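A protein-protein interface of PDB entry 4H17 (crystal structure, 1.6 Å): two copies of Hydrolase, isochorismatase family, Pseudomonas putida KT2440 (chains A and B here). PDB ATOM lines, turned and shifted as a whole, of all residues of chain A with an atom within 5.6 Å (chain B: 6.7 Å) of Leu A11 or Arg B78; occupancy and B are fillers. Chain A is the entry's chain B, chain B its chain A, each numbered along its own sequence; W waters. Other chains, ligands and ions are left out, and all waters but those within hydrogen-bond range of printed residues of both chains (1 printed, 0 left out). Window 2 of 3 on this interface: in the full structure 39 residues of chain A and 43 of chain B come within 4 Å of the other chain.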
ATOM      1  N   THR A   6      -3.794   7.044 -11.865  1.00  0.00           N
ATOM      2  CA  THR A   6      -5.034   7.569 -12.411  1.00  0.00           C
ATOM      3  C   THR A   6      -5.463   6.644 -13.563  1.00  0.00           C
ATOM      4  O   THR A   6      -4.775   5.643 -13.924  1.00  0.00           O
ATOM      5  CB  THR A   6      -4.884   9.037 -12.866  1.00  0.00           C
ATOM      6  OG1 THR A   6      -6.175   9.624 -13.033  1.00  0.00           O
ATOM      7  CG2 THR A   6      -4.146   9.109 -14.169  1.00  0.00           C
ATOM      8  N   THR A   7      -6.636   6.921 -14.101  1.00  0.00           N
ATOM      9  CA  THR A   7      -7.181   6.185 -15.265  1.00  0.00           C
ATOM     10  C   THR A   7      -7.151   7.044 -16.529  1.00  0.00           C
ATOM     11  O   THR A   7      -7.106   8.267 -16.447  1.00  0.00           O
ATOM     12  CB  THR A   7      -8.624   5.780 -14.989  1.00  0.00           C
ATOM     13  OG1 THR A   7      -9.413   6.956 -14.812  1.00  0.00           O
ATOM     14  CG2 THR A   7      -8.747   4.880 -13.717  1.00  0.00           C
ATOM     15  N   MET A   8      -7.123   6.408 -17.702  1.00  0.00           N
ATOM     16  CA  MET A   8      -7.328   7.126 -18.998  1.00  0.00           C
ATOM     17  C   MET A   8      -8.631   7.868 -18.949  1.00  0.00           C
ATOM     18  O   MET A   8      -8.726   8.987 -19.426  1.00  0.00           O
ATOM     19  CB  MET A   8      -7.325   6.124 -20.151  1.00  0.00           C
ATOM     20  CG  MET A   8      -7.389   6.808 -21.533  1.00  0.00           C
ATOM     21  SD  MET A   8      -5.922   8.091 -21.867  1.00  0.00           S
ATOM     22  CE  MET A   8      -4.568   6.943 -22.712  1.00  0.00           C
ATOM     23  N   PHE A   9      -9.677   7.231 -18.417  1.00  0.00           N
ATOM     24  CA  PHE A   9     -10.976   7.910 -18.249  1.00  0.00           C
ATOM     25  C   PHE A   9     -10.783   9.283 -17.584  1.00  0.00           C
ATOM     26  O   PHE A   9     -11.285  10.319 -18.070  1.00  0.00           O
ATOM     27  CB  PHE A   9     -11.925   7.112 -17.379  1.00  0.00           C
ATOM     28  CG  PHE A   9     -12.698   5.995 -18.038  1.00  0.00           C
ATOM     29  CD1 PHE A   9     -13.566   6.241 -19.098  1.00  0.00           C
ATOM     30  CD2 PHE A   9     -12.698   4.722 -17.450  1.00  0.00           C
ATOM     31  CE1 PHE A   9     -14.360   5.223 -19.588  1.00  0.00           C
ATOM     32  CE2 PHE A   9     -13.501   3.703 -17.937  1.00  0.00           C
ATOM     33  CZ  PHE A   9     -14.338   3.972 -19.010  1.00  0.00           C
ATOM     34  N   ARG A  10     -10.114   9.320 -16.443  1.00  0.00           N
ATOM     35  CA  ARG A  10      -9.991  10.572 -15.664  1.00  0.00           C
ATOM     36  C   ARG A  10      -9.081  11.572 -16.366  1.00  0.00           C
ATOM     37  O   ARG A  10      -9.371  12.771 -16.346  1.00  0.00           O
ATOM     38  CB  ARG A  10      -9.567  10.327 -14.228  1.00  0.00           C
ATOM     39  CG  ARG A  10     -10.752   9.868 -13.424  1.00  0.00           C
ATOM     40  CD  ARG A  10     -10.568   9.982 -11.932  1.00  0.00           C
ATOM     41  NE  ARG A  10     -10.068  11.277 -11.531  1.00  0.00           N
ATOM     42  CZ  ARG A  10     -10.743  12.181 -10.796  1.00  0.00           C
ATOM     43  NH1 ARG A  10     -11.988  11.941 -10.401  1.00  0.00           N
ATOM     44  NH2 ARG A  10     -10.166  13.325 -10.466  1.00  0.00           N
ATOM     45  N   LEU A  11      -8.024  11.074 -16.988  1.00  0.00           N
ATOM     46  CA  LEU A  11      -7.103  11.947 -17.708  1.00  0.00           C
ATOM     47  C   LEU A  11      -7.751  12.714 -18.848  1.00  0.00           C
ATOM     48  O   LEU A  11      -7.340  13.846 -19.105  1.00  0.00           O
ATOM     49  CB  LEU A  11      -5.911  11.148 -18.262  1.00  0.00           C
ATOM     50  CG  LEU A  11      -4.919  10.708 -17.160  1.00  0.00           C
ATOM     51  CD1 LEU A  11      -3.943   9.647 -17.619  1.00  0.00           C
ATOM     52  CD2 LEU A  11      -4.165  11.921 -16.586  1.00  0.00           C
ATOM     53  N   THR A  12      -8.715  12.082 -19.522  1.00  0.00           N
ATOM     54  CA  THR A  12      -9.428  12.661 -20.662  1.00  0.00           C
ATOM     55  C   THR A  12     -10.770  13.317 -20.288  1.00  0.00           C
ATOM     56  O   THR A  12     -11.417  13.971 -21.113  1.00  0.00           O
ATOM     57  CB  THR A  12      -9.600  11.616 -21.761  1.00  0.00           C
ATOM     58  OG1 THR A  12     -10.436  10.546 -21.279  1.00  0.00           O
ATOM     59  CG2 THR A  12      -8.254  11.080 -22.230  1.00  0.00           C
ATOM     60  N   GLY A  13     -11.164  13.141 -19.043  1.00  0.00           N
ATOM     61  CA  GLY A  13     -12.411  13.653 -18.521  1.00  0.00           C
ATOM     62  C   GLY A  13     -13.610  12.900 -19.065  1.00  0.00           C
ATOM     63  O   GLY A  13     -14.725  13.429 -19.118  1.00  0.00           O
ATOM     64  N   GLU B  34       3.436  11.371 -26.059  1.00  0.00           N
ATOM     65  CA  GLU B  34       2.609  11.315 -24.863  1.00  0.00           C
ATOM     66  C   GLU B  34       3.093  10.226 -23.913  1.00  0.00           C
ATOM     67  O   GLU B  34       3.124  10.438 -22.704  1.00  0.00           O
ATOM     68  CB  GLU B  34       1.155  11.051 -25.255  1.00  0.00           C
ATOM     69  CG  GLU B  34       0.203  10.949 -24.077  1.00  0.00           C
ATOM     70  CD  GLU B  34      -0.067  12.259 -23.355  1.00  0.00           C
ATOM     71  OE1 GLU B  34      -0.403  13.266 -24.017  1.00  0.00           O
ATOM     72  OE2 GLU B  34       0.039  12.317 -22.116  1.00  0.00           O
ATOM     73  N   SER B  37       6.583  10.511 -21.107  1.00  0.00           N
ATOM     74  CA  SER B  37       6.636  11.292 -19.893  1.00  0.00           C
ATOM     75  C   SER B  37       5.217  11.478 -19.327  1.00  0.00           C
ATOM     76  O   SER B  37       4.255  11.116 -19.973  1.00  0.00           O
ATOM     77  CB  SER B  37       7.306  12.647 -20.163  1.00  0.00           C
ATOM     78  OG  SER B  37       6.435  13.476 -20.917  1.00  0.00           O
ATOM     79  N   GLY B  38       5.100  12.053 -18.135  1.00  0.00           N
ATOM     80  CA  GLY B  38       3.798  12.290 -17.480  1.00  0.00           C
ATOM     81  C   GLY B  38       3.083  11.031 -16.971  1.00  0.00           C
ATOM     82  O   GLY B  38       3.688   9.981 -16.862  1.00  0.00           O
ATOM     83  N   PRO B  39       1.777  11.150 -16.644  1.00  0.00           N
ATOM     84  CA  PRO B  39       0.998  10.038 -16.108  1.00  0.00           C
ATOM     85  C   PRO B  39       0.872   8.877 -17.082  1.00  0.00           C
ATOM     86  O   PRO B  39       0.634   7.734 -16.648  1.00  0.00           O
ATOM     87  CB  PRO B  39      -0.389  10.666 -15.827  1.00  0.00           C
ATOM     88  CG  PRO B  39      -0.428  11.891 -16.645  1.00  0.00           C
ATOM     89  CD  PRO B  39       0.980  12.372 -16.793  1.00  0.00           C
ATOM     90  N   LEU B  40       1.017   9.126 -18.389  1.00  0.00           N
ATOM     91  CA  LEU B  40       0.920   8.047 -19.381  1.00  0.00           C
ATOM     92  C   LEU B  40       2.310   7.533 -19.797  1.00  0.00           C
ATOM     93  O   LEU B  40       2.429   6.803 -20.741  1.00  0.00           O
ATOM     94  CB  LEU B  40       0.078   8.452 -20.602  1.00  0.00           C
ATOM     95  CG  LEU B  40      -1.370   8.773 -20.265  1.00  0.00           C
ATOM     96  CD1 LEU B  40      -1.998   9.321 -21.529  1.00  0.00           C
ATOM     97  CD2 LEU B  40      -2.096   7.515 -19.773  1.00  0.00           C
ATOM     98  N   HIS B  71      -3.537   8.864 -32.125  1.00  0.00           N
ATOM     99  CA  HIS B  71      -4.679   9.537 -31.535  1.00  0.00           C
ATOM    100  C   HIS B  71      -4.983  10.835 -32.255  1.00  0.00           C
ATOM    101  O   HIS B  71      -4.061  11.597 -32.620  1.00  0.00           O
ATOM    102  CB  HIS B  71      -4.425   9.877 -30.093  1.00  0.00           C
ATOM    103  CG  HIS B  71      -4.480   8.722 -29.160  1.00  0.00           C
ATOM    104  ND1 HIS B  71      -5.229   8.726 -28.008  1.00  0.00           N
ATOM    105  CD2 HIS B  71      -3.845   7.538 -29.195  1.00  0.00           C
ATOM    106  CE1 HIS B  71      -5.094   7.568 -27.396  1.00  0.00           C
ATOM    107  NE2 HIS B  71      -4.217   6.848 -28.071  1.00  0.00           N
ATOM    108  N   LEU B  72      -6.270  11.110 -32.422  1.00  0.00           N
ATOM    109  CA  LEU B  72      -6.677  12.456 -32.792  1.00  0.00           C
ATOM    110  C   LEU B  72      -6.255  13.440 -31.700  1.00  0.00           C
ATOM    111  O   LEU B  72      -5.747  14.523 -32.015  1.00  0.00           O
ATOM    112  CB  LEU B  72      -8.171  12.520 -33.017  1.00  0.00           C
ATOM    113  CG  LEU B  72      -8.604  11.974 -34.369  1.00  0.00           C
ATOM    114  CD1 LEU B  72     -10.096  11.673 -34.316  1.00  0.00           C
ATOM    115  CD2 LEU B  72      -8.283  12.972 -35.480  1.00  0.00           C
ATOM    116  N   GLY B  73      -6.381  13.049 -30.436  1.00  0.00           N
ATOM    117  CA  GLY B  73      -6.031  13.960 -29.332  1.00  0.00           C
ATOM    118  C   GLY B  73      -6.902  15.185 -29.159  1.00  0.00           C
ATOM    119  O   GLY B  73      -7.895  15.430 -29.890  1.00  0.00           O
ATOM    120  N   THR B  74      -6.473  15.989 -28.199  1.00  0.00           N
ATOM    121  CA  THR B  74      -7.169  17.205 -27.839  1.00  0.00           C
ATOM    122  C   THR B  74      -6.145  18.343 -27.819  1.00  0.00           C
ATOM    123  O   THR B  74      -5.138  18.220 -27.200  1.00  0.00           O
ATOM    124  CB  THR B  74      -7.819  17.049 -26.445  1.00  0.00           C
ATOM    125  OG1 THR B  74      -8.732  15.938 -26.430  1.00  0.00           O
ATOM    126  CG2 THR B  74      -8.603  18.255 -26.042  1.00  0.00           C
ATOM    127  N   VAL B  75      -6.457  19.439 -28.509  1.00  0.00           N
ATOM    128  CA  VAL B  75      -5.660  20.649 -28.469  1.00  0.00           C
ATOM    129  C   VAL B  75      -5.589  21.102 -27.019  1.00  0.00           C
ATOM    130  O   VAL B  75      -6.609  21.273 -26.310  1.00  0.00           O
ATOM    131  CB  VAL B  75      -6.226  21.758 -29.355  1.00  0.00           C
ATOM    132  CG1 VAL B  75      -5.456  23.045 -29.104  1.00  0.00           C
ATOM    133  CG2 VAL B  75      -6.158  21.324 -30.810  1.00  0.00           C
ATOM    134  N   GLY B  76      -4.363  21.298 -26.565  1.00  0.00           N
ATOM    135  CA  GLY B  76      -4.069  21.635 -25.169  1.00  0.00           C
ATOM    136  C   GLY B  76      -4.193  20.512 -24.165  1.00  0.00           C
ATOM    137  O   GLY B  76      -4.031  20.717 -22.974  1.00  0.00           O
ATOM    138  N   GLY B  77      -4.456  19.318 -24.653  1.00  0.00           N
ATOM    139  CA  GLY B  77      -4.803  18.177 -23.792  1.00  0.00           C
ATOM    140  C   GLY B  77      -3.936  16.980 -24.058  1.00  0.00           C
ATOM    141  O   GLY B  77      -2.807  17.087 -24.520  1.00  0.00           O
ATOM    142  N   ARG B  78      -4.449  15.800 -23.741  1.00  0.00           N
ATOM    143  CA  ARG B  78      -3.714  14.590 -23.971  1.00  0.00           C
ATOM    144  C   ARG B  78      -3.557  14.295 -25.472  1.00  0.00           C
ATOM    145  O   ARG B  78      -4.474  14.544 -26.256  1.00  0.00           O
ATOM    146  CB  ARG B  78      -4.407  13.430 -23.216  1.00  0.00           C
ATOM    147  CG  ARG B  78      -4.419  13.583 -21.685  1.00  0.00           C
ATOM    148  CD  ARG B  78      -3.033  13.401 -21.094  1.00  0.00           C
ATOM    149  NE  ARG B  78      -2.956  13.909 -19.727  1.00  0.00           N
ATOM    150  CZ  ARG B  78      -1.827  14.188 -19.074  1.00  0.00           C
ATOM    151  NH1 ARG B  78      -0.626  13.994 -19.627  1.00  0.00           N
ATOM    152  NH2 ARG B  78      -1.902  14.646 -17.843  1.00  0.00           N
ATOM    153  N   PHE B  79      -2.388  13.791 -25.859  1.00  0.00           N
ATOM    154  CA  PHE B  79      -2.008  13.554 -27.251  1.00  0.00           C
ATOM    155  C   PHE B  79      -2.214  14.801 -28.107  1.00  0.00           C
ATOM    156  O   PHE B  79      -2.532  14.712 -29.283  1.00  0.00           O
ATOM    157  CB  PHE B  79      -2.807  12.372 -27.860  1.00  0.00           C
ATOM    158  CG  PHE B  79      -2.727  11.092 -27.031  1.00  0.00           C
ATOM    159  CD1 PHE B  79      -3.545  10.866 -25.946  1.00  0.00           C
ATOM    160  CD2 PHE B  79      -1.742  10.131 -27.337  1.00  0.00           C
ATOM    161  CE1 PHE B  79      -3.444   9.708 -25.189  1.00  0.00           C
ATOM    162  CE2 PHE B  79      -1.639   8.963 -26.579  1.00  0.00           C
ATOM    163  CZ  PHE B  79      -2.476   8.764 -25.501  1.00  0.00           C
ATOM    164  N   ASP B  80      -1.977  15.965 -27.499  1.00  0.00           N
ATOM    165  CA  ASP B  80      -2.196  17.246 -28.141  1.00  0.00           C
ATOM    166  C   ASP B  80      -1.610  17.311 -29.569  1.00  0.00           C
ATOM    167  O   ASP B  80      -0.395  17.294 -29.728  1.00  0.00           O
ATOM    168  CB  ASP B  80      -1.517  18.283 -27.271  1.00  0.00           C
ATOM    169  CG  ASP B  80      -1.718  19.691 -27.742  1.00  0.00           C
ATOM    170  OD1 ASP B  80      -2.326  19.925 -28.792  1.00  0.00           O
ATOM    171  OD2 ASP B  80      -1.191  20.578 -27.027  1.00  0.00           O
ATOM    172  N   PRO B  81      -2.456  17.493 -30.592  1.00  0.00           N
ATOM    173  CA  PRO B  81      -1.926  17.474 -31.933  1.00  0.00           C
ATOM    174  C   PRO B  81      -1.214  18.761 -32.331  1.00  0.00           C
ATOM    175  O   PRO B  81      -0.544  18.784 -33.353  1.00  0.00           O
ATOM    176  CB  PRO B  81      -3.140  17.222 -32.776  1.00  0.00           C
ATOM    177  CG  PRO B  81      -4.266  17.889 -32.004  1.00  0.00           C
ATOM    178  CD  PRO B  81      -3.926  17.589 -30.573  1.00  0.00           C
ATOM    179  N   ALA B  85       3.157  16.190 -27.337  1.00  0.00           N
ATOM    180  CA  ALA B  85       2.593  14.861 -27.019  1.00  0.00           C
ATOM    181  C   ALA B  85       1.982  14.147 -28.231  1.00  0.00           C
ATOM    182  O   ALA B  85       1.963  12.916 -28.273  1.00  0.00           O
ATOM    183  CB  ALA B  85       1.531  15.011 -25.924  1.00  0.00           C
ATOM    184  N   GLY B  86       1.457  14.902 -29.198  1.00  0.00           N
ATOM    185  CA  GLY B  86       0.904  14.299 -30.389  1.00  0.00           C
ATOM    186  C   GLY B  86       1.926  13.865 -31.437  1.00  0.00           C
ATOM    187  O   GLY B  86       1.565  13.185 -32.395  1.00  0.00           O
ATOM    188  N   ARG B 161       1.515   0.621 -18.853  1.00  0.00           N
ATOM    189  CA  ARG B 161       1.916   1.273 -17.600  1.00  0.00           C
ATOM    190  C   ARG B 161       1.327   0.572 -16.364  1.00  0.00           C
ATOM    191  O   ARG B 161       0.471  -0.318 -16.466  1.00  0.00           O
ATOM    192  CB  ARG B 161       1.541   2.731 -17.653  1.00  0.00           C
ATOM    193  CG  ARG B 161       0.038   3.003 -17.486  1.00  0.00           C
ATOM    194  CD  ARG B 161      -0.331   4.469 -17.700  1.00  0.00           C
ATOM    195  NE  ARG B 161      -1.576   4.856 -17.004  1.00  0.00           N
ATOM    196  CZ  ARG B 161      -2.808   4.502 -17.367  1.00  0.00           C
ATOM    197  NH1 ARG B 161      -3.024   3.761 -18.457  1.00  0.00           N
ATOM    198  NH2 ARG B 161      -3.823   4.911 -16.617  1.00  0.00           N
HETATM  199  O   HOH W   1      -5.004  15.096 -18.322  1.00  0.00           O
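The guanidinium group of Arg B161 is in hydrogen-bond range of the backbone carbonyl oxygen of Thr A6 (2.9 Å).
OE2 of Glu B34 is in salt-bridge range of NH1 of Arg B78, 3.1 Å away. The side-chain carboxylate (OE1) of Glu B34 is in hydrogen-bond range of the backbone NH (N) of Phe B79, 2.8 Å away. OG1 of Thr A7 sits at hydrogen-bond distance from N of Arg A10 (3.0 Å). The side-chain hydroxyl (OG1) of Thr A12 is in hydrogen-bond range of the backbone carbonyl oxygen (O) of Met A8, 3.0 Å away.
Among the printed residues, merely in contact across the chains: Leu A11 with Leu B40, Met A8 with Leu B40, Leu A11 with Pro B39, Leu A11 with Arg B78, Met A8 with Arg B161, Thr A7 with Arg B161 and Met A8 with Phe B79.
Printed residues of chain B within 4 Å of Thr A7: Arg B161. Printed residues of chain B within 4 Å of Leu A11: Pro B39 (3.7 Å), Leu B40 (3.5 Å) and Arg B78 (3.8 Å). Printed residues of chain A within 4 Å of Pro B39: Leu A11. Of the printed residues of chain A, Leu B40 touches Met A8 (3.7 Å) and Leu A11 (3.5 Å). Arg B78 touches just one residue of chain A: Leu A11. Of the printed residues of chain A, Phe B79 touches Met A8 (3.9 Å). Gly B86 touches none of the printed residues of chain A. The nearest residue of chain A that does not touch Arg B78 is Thr A12 (4.6 Å). The nearest printed residue of chain A that does not touch Arg B161 is Leu A11 (4.8 Å).
Printed residues of chain B that touch a printed residue of chain A: Pro B39, Leu B40, Arg B78, Phe B79 and Arg B161. Of the 8 printed residues of chain A, 4 touch a printed residue of chain B. Among the printed residues, 8 pairs touch across the chains.
No position is printed for both chains. Of the 8 pairs that touch across the chains among the printed residues, none has its exchanged pair printed and touching as well.
Water W1 lies within hydrogen-bond range of NE of Arg B78 and O of Leu A11.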
